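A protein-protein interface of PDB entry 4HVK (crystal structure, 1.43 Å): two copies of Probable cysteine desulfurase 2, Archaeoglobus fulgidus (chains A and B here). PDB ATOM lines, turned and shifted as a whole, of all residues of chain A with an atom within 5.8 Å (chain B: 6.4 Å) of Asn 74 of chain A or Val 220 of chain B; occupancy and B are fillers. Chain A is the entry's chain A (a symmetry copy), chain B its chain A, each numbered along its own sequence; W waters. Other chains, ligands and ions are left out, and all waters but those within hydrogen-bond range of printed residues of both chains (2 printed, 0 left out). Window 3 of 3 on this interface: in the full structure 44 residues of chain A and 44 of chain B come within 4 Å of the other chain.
The backbone carbonyl oxygen (O) of Leu 222 of chain B sits at hydrogen-bond distance from the side-chain amide nitrogen (ND2) of Asn 74 of chain A (2.8 Å).
The side-chain carboxylate (OE2) of Glu 71 of chain B is in salt-bridge range of the guanidinium group (NE) of Arg 231 of chain B, at 2.9 Å.
The backbone NH of Ser 232 of chain B is in hydrogen-bond range of the backbone carbonyl oxygen of Ile 221 of chain B.
The side-chain hydroxyl (OG) of Ser 232 of chain B sits at hydrogen-bond distance from the backbone NH (N) of Gly 223 of chain B, 3.1 Å away.
O of Thr 70 of chain A lies within hydrogen-bond range of ND2 of Asn 74 of chain A, 2.9 Å away.
The side-chain hydroxyl (OG) of Ser 100 of chain A sits at hydrogen-bond distance from the side-chain amide oxygen (OD1) of Asn 73 of chain A (2.9 Å).
Leu 222 of chain B touches Thr 70 of chain A.
OD1 of Asn 74 of chain A touches O of Val 220 of chain B, at 3.6 Å.
Ile 221 of chain B touches Asn 74 of chain A (CA to OD1, 3.6 Å).
Leu 222 of chain B touches Ser 100 of chain A (O to CA, 3.7 Å).
CA of Ser 100 of chain A touches CA of Gly 223 of chain B, 3.7 Å away.
CA of Pro 104 of chain A touches CD1 of Leu 222 of chain B (3.97 Å).
Asn 74 of chain B touches Val 220 of chain A.
Val 220 of chain A touches Val 220 of chain B (CG1 to CG1, 3.8 Å).
CD1 of Ile 221 of chain A touches CG of Glu 71 of chain B, 3.9 Å away.
Asn 74 of chain B touches Ile 221 of chain A (OD1 to CA, 3.6 Å).
Of the printed residues of chain B, Asn 74 of chain A touches Val 220, Ile 221 and Leu 222.
Of the printed residues of chain A, Val 220 of chain B touches Asn 74 and Val 220.
Printed residues of chain B within 4 Å of Pro 104 of chain A: Leu 222.
Of the printed residues of chain A, Leu 222 of chain B touches Thr 70 (3.4 Å), Asn 74 (2.8 Å), Ser 100 (3.7 Å) and Pro 104 (3.97 Å).
Val 101 of chain A touches none of the printed residues of chain B.
Leu 75 of chain B touches none of the printed residues of chain A.
The nearest printed residue of chain A that does not touch Val 220 of chain B is Ile 221 of chain A (4.7 Å).
The nearest printed residue of chain A that does not touch Glu 71 of chain B is Glu 71 of chain A (5.4 Å).
Printed residues of chain B that touch a printed residue of chain A: Glu 71, Asn 74, Val 220, Ile 221, Leu 222, Gly 223 and Ser 232.
Of the 16 printed residues of chain A, 7 touch a printed residue of chain B.
Among the printed residues, 14 pairs touch across the chains.
Among the printed residues, no Asp or Glu carboxylate lies within 4 Å of a Lys or Arg side-chain nitrogen of the other chain.
Glu 71 of chain A touches Ile 221 of chain B, and with the chains exchanged Ile 221 of chain A touches Glu 71 of chain B.
Asn 74 of chain A touches Val 220 of chain B, and with the chains exchanged Val 220 of chain A touches Asn 74 of chain B.
Asn 74 of chain A touches Ile 221 of chain B, and with the chains exchanged Ile 221 of chain A touches Asn 74 of chain B.
Val 220 of chain A touches its own counterpart, Val 220 of chain B.
Of the 14 pairs that touch across the chains among the printed residues, 7 have their exchanged pair printed and touching as well.
Water W1 bridges the backbone carbonyl oxygen (O) of Val 220 of chain B (2.7 Å) and the side-chain amide oxygen (OD1) of Asn 74 of chain A (2.8 Å).
Water W2 lies within hydrogen-bond range of the backbone carbonyl oxygen of Val 220 of chain A (2.7 Å) and the side-chain amide oxygen of Asn 74 of chain B (2.8 Å).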
ATOM      1  N   ALA A  69     -15.751 -13.945  17.438  1.00  0.00           N
ATOM      2  CA  ALA A  69     -15.927 -13.346  16.147  1.00  0.00           C
ATOM      3  C   ALA A  69     -15.938 -11.834  16.261  1.00  0.00           C
ATOM      4  O   ALA A  69     -15.391 -11.181  15.334  1.00  0.00           O
ATOM      5  CB  ALA A  69     -17.207 -13.888  15.496  1.00  0.00           C
ATOM      6  N   THR A  70     -16.559 -11.253  17.248  1.00  0.00           N
ATOM      7  CA  THR A  70     -16.590  -9.771  17.336  1.00  0.00           C
ATOM      8  C   THR A  70     -15.190  -9.237  17.387  1.00  0.00           C
ATOM      9  O   THR A  70     -14.837  -8.298  16.608  1.00  0.00           O
ATOM     10  CB  THR A  70     -17.445  -9.307  18.521  1.00  0.00           C
ATOM     11  OG1 THR A  70     -18.788  -9.647  18.282  1.00  0.00           O
ATOM     12  CG2 THR A  70     -17.323  -7.800  18.744  1.00  0.00           C
ATOM     13  N   GLU A  71     -14.355  -9.707  18.291  1.00  0.00           N
ATOM     14  CA  GLU A  71     -12.997  -9.199  18.404  1.00  0.00           C
ATOM     15  C   GLU A  71     -12.135  -9.484  17.147  1.00  0.00           C
ATOM     16  O   GLU A  71     -11.257  -8.680  16.754  1.00  0.00           O
ATOM     17  CB  GLU A  71     -12.312  -9.729  19.652  1.00  0.00           C
ATOM     18  CG  GLU A  71     -10.890  -9.204  19.868  1.00  0.00           C
ATOM     19  CD  GLU A  71      -9.990 -10.113  20.750  1.00  0.00           C
ATOM     20  OE1 GLU A  71     -10.441 -10.864  21.595  1.00  0.00           O
ATOM     21  OE2 GLU A  71      -8.792 -10.143  20.517  1.00  0.00           O
ATOM     22  N   ALA A  72     -12.382 -10.626  16.488  1.00  0.00           N
ATOM     23  CA  ALA A  72     -11.717 -10.961  15.247  1.00  0.00           C
ATOM     24  C   ALA A  72     -12.117  -9.987  14.147  1.00  0.00           C
ATOM     25  O   ALA A  72     -11.261  -9.530  13.382  1.00  0.00           O
ATOM     26  CB  ALA A  72     -12.008 -12.361  14.811  1.00  0.00           C
ATOM     27  N   ASN A  73     -13.395  -9.645  14.020  1.00  0.00           N
ATOM     28  CA  ASN A  73     -13.804  -8.646  13.035  1.00  0.00           C
ATOM     29  C   ASN A  73     -13.264  -7.299  13.356  1.00  0.00           C
ATOM     30  O   ASN A  73     -12.894  -6.590  12.400  1.00  0.00           O
ATOM     31  CB  ASN A  73     -15.338  -8.601  13.017  1.00  0.00           C
ATOM     32  CG  ASN A  73     -16.002  -9.711  12.224  1.00  0.00           C
ATOM     33  OD1 ASN A  73     -17.278 -10.016  12.498  1.00  0.00           O
ATOM     34  ND2 ASN A  73     -15.343 -10.273  11.290  1.00  0.00           N
ATOM     35  N   ASN A  74     -13.169  -6.874  14.599  1.00  0.00           N
ATOM     36  CA  ASN A  74     -12.543  -5.649  14.931  1.00  0.00           C
ATOM     37  C   ASN A  74     -11.090  -5.623  14.472  1.00  0.00           C
ATOM     38  O   ASN A  74     -10.568  -4.627  13.945  1.00  0.00           O
ATOM     39  CB  ASN A  74     -12.602  -5.313  16.423  1.00  0.00           C
ATOM     40  CG  ASN A  74     -13.919  -4.772  16.951  1.00  0.00           C
ATOM     41  OD1 ASN A  74     -13.886  -3.648  17.487  1.00  0.00           O
ATOM     42  ND2 ASN A  74     -14.987  -5.357  16.704  1.00  0.00           N
ATOM     43  N   LEU A  75     -10.364  -6.678  14.735  1.00  0.00           N
ATOM     44  CA  LEU A  75      -8.973  -6.818  14.355  1.00  0.00           C
ATOM     45  C   LEU A  75      -8.826  -6.715  12.861  1.00  0.00           C
ATOM     46  O   LEU A  75      -7.941  -6.007  12.333  1.00  0.00           O
ATOM     47  CB  LEU A  75      -8.378  -8.095  14.908  1.00  0.00           C
ATOM     48  CG  LEU A  75      -6.930  -8.423  14.540  1.00  0.00           C
ATOM     49  CD1 LEU A  75      -5.930  -7.385  15.073  1.00  0.00           C
ATOM     50  CD2 LEU A  75      -6.532  -9.772  15.118  1.00  0.00           C
ATOM     51  N   ALA A  76      -9.650  -7.422  12.099  1.00  0.00           N
ATOM     52  CA  ALA A  76      -9.604  -7.440  10.649  1.00  0.00           C
ATOM     53  C   ALA A  76      -9.770  -6.035  10.124  1.00  0.00           C
ATOM     54  O   ALA A  76      -9.005  -5.604   9.296  1.00  0.00           O
ATOM     55  CB  ALA A  76     -10.671  -8.354  10.048  1.00  0.00           C
ATOM     56  N   ILE A  77     -10.805  -5.349  10.551  1.00  0.00           N
ATOM     57  CA  ILE A  77     -11.161  -4.038   9.985  1.00  0.00           C
ATOM     58  C   ILE A  77     -10.205  -3.009  10.454  1.00  0.00           C
ATOM     59  O   ILE A  77      -9.565  -2.279   9.614  1.00  0.00           O
ATOM     60  CB  ILE A  77     -12.650  -3.645  10.278  1.00  0.00           C
ATOM     61  CG1 ILE A  77     -13.588  -4.714   9.684  1.00  0.00           C
ATOM     62  CG2 ILE A  77     -12.977  -2.248   9.749  1.00  0.00           C
ATOM     63  CD1 ILE A  77     -13.572  -4.906   8.163  1.00  0.00           C
ATOM     64  N   ILE A  78     -10.125  -2.793  11.754  1.00  0.00           N
ATOM     65  CA  ILE A  78      -9.302  -1.724  12.266  1.00  0.00           C
ATOM     66  C   ILE A  78      -7.819  -2.053  12.152  1.00  0.00           C
ATOM     67  O   ILE A  78      -7.001  -1.208  11.774  1.00  0.00           O
ATOM     68  CB  ILE A  78      -9.666  -1.364  13.745  1.00  0.00           C
ATOM     69  CG1 ILE A  78     -11.108  -0.852  13.779  1.00  0.00           C
ATOM     70  CG2 ILE A  78      -8.648  -0.373  14.357  1.00  0.00           C
ATOM     71  CD1 ILE A  78     -11.748  -0.871  15.189  1.00  0.00           C
ATOM     72  N   GLY A  79      -7.432  -3.299  12.522  1.00  0.00           N
ATOM     73  CA  GLY A  79      -6.035  -3.668  12.482  1.00  0.00           C
ATOM     74  C   GLY A  79      -5.466  -3.621  11.101  1.00  0.00           C
ATOM     75  O   GLY A  79      -4.349  -3.134  10.903  1.00  0.00           O
ATOM     76  N   SER A 100     -20.387  -6.033  14.212  1.00  0.00           N
ATOM     77  CA  SER A 100     -18.966  -6.106  14.548  1.00  0.00           C
ATOM     78  C   SER A 100     -18.007  -5.858  13.419  1.00  0.00           C
ATOM     79  O   SER A 100     -16.818  -5.801  13.657  1.00  0.00           O
ATOM     80  CB  SER A 100     -18.643  -7.433  15.265  1.00  0.00           C
ATOM     81  OG  SER A 100     -18.866  -8.556  14.366  1.00  0.00           O
ATOM     82  N   VAL A 101     -18.543  -5.740  12.181  1.00  0.00           N
ATOM     83  CA  VAL A 101     -17.830  -5.125  11.054  1.00  0.00           C
ATOM     84  C   VAL A 101     -18.249  -3.717  10.796  1.00  0.00           C
ATOM     85  O   VAL A 101     -17.385  -2.851  10.654  1.00  0.00           O
ATOM     86  CB  VAL A 101     -18.008  -5.979   9.763  1.00  0.00           C
ATOM     87  CG1 VAL A 101     -17.495  -5.231   8.569  1.00  0.00           C
ATOM     88  CG2 VAL A 101     -17.402  -7.379   9.952  1.00  0.00           C
ATOM     89  N   PRO A 104     -16.857  -1.072  13.603  1.00  0.00           N
ATOM     90  CA  PRO A 104     -15.462  -0.765  13.343  1.00  0.00           C
ATOM     91  C   PRO A 104     -15.307   0.115  12.078  1.00  0.00           C
ATOM     92  O   PRO A 104     -14.445   1.030  12.052  1.00  0.00           O
ATOM     93  CB  PRO A 104     -14.842  -2.133  13.174  1.00  0.00           C
ATOM     94  CG  PRO A 104     -15.626  -2.958  14.107  1.00  0.00           C
ATOM     95  CD  PRO A 104     -17.044  -2.486  13.953  1.00  0.00           C
ATOM     96  N   VAL A 220      -4.875  -4.689  18.113  1.00  0.00           N
ATOM     97  CA  VAL A 220      -5.738  -3.771  18.886  1.00  0.00           C
ATOM     98  C   VAL A 220      -5.487  -4.003  20.348  1.00  0.00           C
ATOM     99  O   VAL A 220      -5.401  -2.990  21.110  1.00  0.00           O
ATOM    100  CB  VAL A 220      -7.224  -4.017  18.453  1.00  0.00           C
ATOM    101  CG1 VAL A 220      -8.212  -3.271  19.311  1.00  0.00           C
ATOM    102  CG2 VAL A 220      -7.288  -3.761  16.940  1.00  0.00           C
ATOM    103  N   ILE A 221      -5.387  -5.297  20.747  1.00  0.00           N
ATOM    104  CA  ILE A 221      -5.229  -5.573  22.215  1.00  0.00           C
ATOM    105  C   ILE A 221      -3.723  -5.695  22.518  1.00  0.00           C
ATOM    106  O   ILE A 221      -3.029  -6.511  21.924  1.00  0.00           O
ATOM    107  CB  ILE A 221      -5.948  -6.839  22.695  1.00  0.00           C
ATOM    108  CG1 ILE A 221      -7.458  -6.698  22.442  1.00  0.00           C
ATOM    109  CG2 ILE A 221      -5.700  -7.127  24.185  1.00  0.00           C
ATOM    110  CD1 ILE A 221      -8.172  -5.599  23.245  1.00  0.00           C
ATOM    111  N   GLU B  71      -7.281  -7.142  28.417  1.00  0.00           N
ATOM    112  CA  GLU B  71      -8.289  -6.350  27.730  1.00  0.00           C
ATOM    113  C   GLU B  71      -8.938  -5.272  28.636  1.00  0.00           C
ATOM    114  O   GLU B  71      -9.300  -4.161  28.183  1.00  0.00           O
ATOM    115  CB  GLU B  71      -9.355  -7.234  27.106  1.00  0.00           C
ATOM    116  CG  GLU B  71     -10.431  -6.477  26.324  1.00  0.00           C
ATOM    117  CD  GLU B  71     -11.780  -7.234  26.177  1.00  0.00           C
ATOM    118  OE1 GLU B  71     -11.859  -8.448  26.200  1.00  0.00           O
ATOM    119  OE2 GLU B  71     -12.811  -6.580  26.135  1.00  0.00           O
ATOM    120  N   ASN B  74      -6.434  -2.429  28.776  1.00  0.00           N
ATOM    121  CA  ASN B  74      -6.531  -1.686  27.576  1.00  0.00           C
ATOM    122  C   ASN B  74      -7.720  -0.733  27.603  1.00  0.00           C
ATOM    123  O   ASN B  74      -7.660   0.431  27.176  1.00  0.00           O
ATOM    124  CB  ASN B  74      -6.616  -2.556  26.320  1.00  0.00           C
ATOM    125  CG  ASN B  74      -5.318  -3.171  25.824  1.00  0.00           C
ATOM    126  OD1 ASN B  74      -4.970  -2.881  24.664  1.00  0.00           O
ATOM    127  ND2 ASN B  74      -4.575  -3.791  26.603  1.00  0.00           N
ATOM    128  N   LEU B  75      -8.860  -1.217  28.019  1.00  0.00           N
ATOM    129  CA  LEU B  75     -10.080  -0.442  28.119  1.00  0.00           C
ATOM    130  C   LEU B  75      -9.887   0.721  29.054  1.00  0.00           C
ATOM    131  O   LEU B  75     -10.270   1.873  28.760  1.00  0.00           O
ATOM    132  CB  LEU B  75     -11.254  -1.313  28.514  1.00  0.00           C
ATOM    133  CG  LEU B  75     -12.606  -0.630  28.725  1.00  0.00           C
ATOM    134  CD1 LEU B  75     -13.150   0.023  27.445  1.00  0.00           C
ATOM    135  CD2 LEU B  75     -13.641  -1.644  29.190  1.00  0.00           C
ATOM    136  N   ILE B  78      -6.861   3.205  27.332  1.00  0.00           N
ATOM    137  CA  ILE B  78      -7.232   3.817  26.078  1.00  0.00           C
ATOM    138  C   ILE B  78      -8.663   4.336  26.108  1.00  0.00           C
ATOM    139  O   ILE B  78      -8.958   5.436  25.627  1.00  0.00           O
ATOM    140  CB  ILE B  78      -7.033   2.840  24.872  1.00  0.00           C
ATOM    141  CG1 ILE B  78      -5.545   2.499  24.762  1.00  0.00           C
ATOM    142  CG2 ILE B  78      -7.629   3.418  23.566  1.00  0.00           C
ATOM    143  CD1 ILE B  78      -5.252   1.233  23.919  1.00  0.00           C
ATOM    144  N   GLY B  79      -9.605   3.523  26.647  1.00  0.00           N
ATOM    145  CA  GLY B  79     -10.991   3.931  26.670  1.00  0.00           C
ATOM    146  C   GLY B  79     -11.216   5.163  27.487  1.00  0.00           C
ATOM    147  O   GLY B  79     -11.961   6.056  27.075  1.00  0.00           O
ATOM    148  N   GLN B 218     -14.662   5.335  26.213  1.00  0.00           N
ATOM    149  CA  GLN B 218     -14.919   4.928  24.815  1.00  0.00           C
ATOM    150  C   GLN B 218     -14.704   3.423  24.742  1.00  0.00           C
ATOM    151  O   GLN B 218     -13.714   2.913  25.270  1.00  0.00           O
ATOM    152  CB  GLN B 218     -13.878   5.680  23.937  1.00  0.00           C
ATOM    153  CG  GLN B 218     -14.034   5.505  22.471  1.00  0.00           C
ATOM    154  CD  GLN B 218     -13.091   6.429  21.705  1.00  0.00           C
ATOM    155  OE1 GLN B 218     -13.162   7.661  21.812  1.00  0.00           O
ATOM    156  NE2 GLN B 218     -12.233   5.831  20.936  1.00  0.00           N
ATOM    157  N   PRO B 219     -15.604   2.665  24.115  1.00  0.00           N
ATOM    158  CA  PRO B 219     -15.350   1.256  23.997  1.00  0.00           C
ATOM    159  C   PRO B 219     -14.165   1.002  23.105  1.00  0.00           C
ATOM    160  O   PRO B 219     -13.872   1.843  22.182  1.00  0.00           O
ATOM    161  CB  PRO B 219     -16.541   0.720  23.231  1.00  0.00           C
ATOM    162  CG  PRO B 219     -17.221   1.834  22.733  1.00  0.00           C
ATOM    163  CD  PRO B 219     -16.855   3.044  23.503  1.00  0.00           C
ATOM    164  N   VAL B 220     -13.510  -0.088  23.265  1.00  0.00           N
ATOM    165  CA  VAL B 220     -12.500  -0.464  22.252  1.00  0.00           C
ATOM    166  C   VAL B 220     -13.095  -1.509  21.354  1.00  0.00           C
ATOM    167  O   VAL B 220     -12.883  -1.418  20.104  1.00  0.00           O
ATOM    168  CB  VAL B 220     -11.208  -0.936  23.002  1.00  0.00           C
ATOM    169  CG1 VAL B 220     -10.176  -1.522  22.073  1.00  0.00           C
ATOM    170  CG2 VAL B 220     -10.758   0.240  23.883  1.00  0.00           C
ATOM    171  N   ILE B 221     -13.809  -2.493  21.961  1.00  0.00           N
ATOM    172  CA  ILE B 221     -14.342  -3.608  21.107  1.00  0.00           C
ATOM    173  C   ILE B 221     -15.784  -3.249  20.699  1.00  0.00           C
ATOM    174  O   ILE B 221     -16.634  -3.011  21.548  1.00  0.00           O
ATOM    175  CB  ILE B 221     -14.333  -4.980  21.791  1.00  0.00           C
ATOM    176  CG1 ILE B 221     -12.888  -5.363  22.151  1.00  0.00           C
ATOM    177  CG2 ILE B 221     -14.955  -6.079  20.914  1.00  0.00           C
ATOM    178  CD1 ILE B 221     -11.940  -5.591  20.964  1.00  0.00           C
ATOM    179  N   LEU B 222     -15.968  -3.011  19.397  1.00  0.00           N
ATOM    180  CA  LEU B 222     -17.167  -2.487  18.808  1.00  0.00           C
ATOM    181  C   LEU B 222     -18.015  -3.577  18.155  1.00  0.00           C
ATOM    182  O   LEU B 222     -17.494  -4.558  17.615  1.00  0.00           O
ATOM    183  CB  LEU B 222     -16.783  -1.400  17.800  1.00  0.00           C
ATOM    184  CG  LEU B 222     -15.881  -0.271  18.250  1.00  0.00           C
ATOM    185  CD1 LEU B 222     -15.434   0.563  17.088  1.00  0.00           C
ATOM    186  CD2 LEU B 222     -16.593   0.497  19.332  1.00  0.00           C
ATOM    187  N   GLY B 223     -19.331  -3.414  18.175  1.00  0.00           N
ATOM    188  CA  GLY B 223     -20.204  -4.427  17.639  1.00  0.00           C
ATOM    189  C   GLY B 223     -21.616  -4.264  18.125  1.00  0.00           C
ATOM    190  O   GLY B 223     -22.209  -3.204  17.989  1.00  0.00           O
ATOM    191  N   LEU B 230     -20.114  -0.762  26.085  1.00  0.00           N
ATOM    192  CA  LEU B 230     -18.722  -0.621  26.342  1.00  0.00           C
ATOM    193  C   LEU B 230     -17.789  -1.731  25.860  1.00  0.00           C
ATOM    194  O   LEU B 230     -16.578  -1.586  25.803  1.00  0.00           O
ATOM    195  CB  LEU B 230     -18.422  -0.362  27.860  1.00  0.00           C
ATOM    196  CG  LEU B 230     -18.733   1.000  28.373  1.00  0.00           C
ATOM    197  CD1 LEU B 230     -18.352   1.055  29.834  1.00  0.00           C
ATOM    198  CD2 LEU B 230     -17.832   1.940  27.516  1.00  0.00           C
ATOM    199  N   ARG B 231     -18.400  -2.915  25.633  1.00  0.00           N
ATOM    200  CA  ARG B 231     -17.621  -4.099  25.252  1.00  0.00           C
ATOM    201  C   ARG B 231     -18.514  -5.063  24.534  1.00  0.00           C
ATOM    202  O   ARG B 231     -19.247  -5.844  25.143  1.00  0.00           O
ATOM    203  CB  ARG B 231     -16.931  -4.665  26.492  1.00  0.00           C
ATOM    204  CG  ARG B 231     -15.825  -5.667  26.190  1.00  0.00           C
ATOM    205  CD  ARG B 231     -16.351  -7.082  26.046  1.00  0.00           C
ATOM    206  NE  ARG B 231     -15.262  -8.004  25.773  1.00  0.00           N
ATOM    207  CZ  ARG B 231     -15.434  -9.281  25.499  1.00  0.00           C
ATOM    208  NH1 ARG B 231     -16.668  -9.749  25.375  1.00  0.00           N
ATOM    209  NH2 ARG B 231     -14.405 -10.059  25.320  1.00  0.00           N
ATOM    210  N   SER B 232     -18.516  -4.994  23.202  1.00  0.00           N
ATOM    211  CA  SER B 232     -19.415  -5.803  22.407  1.00  0.00           C
ATOM    212  C   SER B 232     -18.893  -7.234  22.278  1.00  0.00           C
ATOM    213  O   SER B 232     -17.744  -7.522  22.540  1.00  0.00           O
ATOM    214  CB  SER B 232     -19.577  -5.188  21.042  1.00  0.00           C
ATOM    215  OG  SER B 232     -20.357  -4.007  21.026  1.00  0.00           O
HETATM  216  O   HOH W   1     -11.370  -2.749  18.312  1.00  0.00           O
HETATM  217  O   HOH W   2      -6.971  -1.867  22.994  1.00  0.00           O
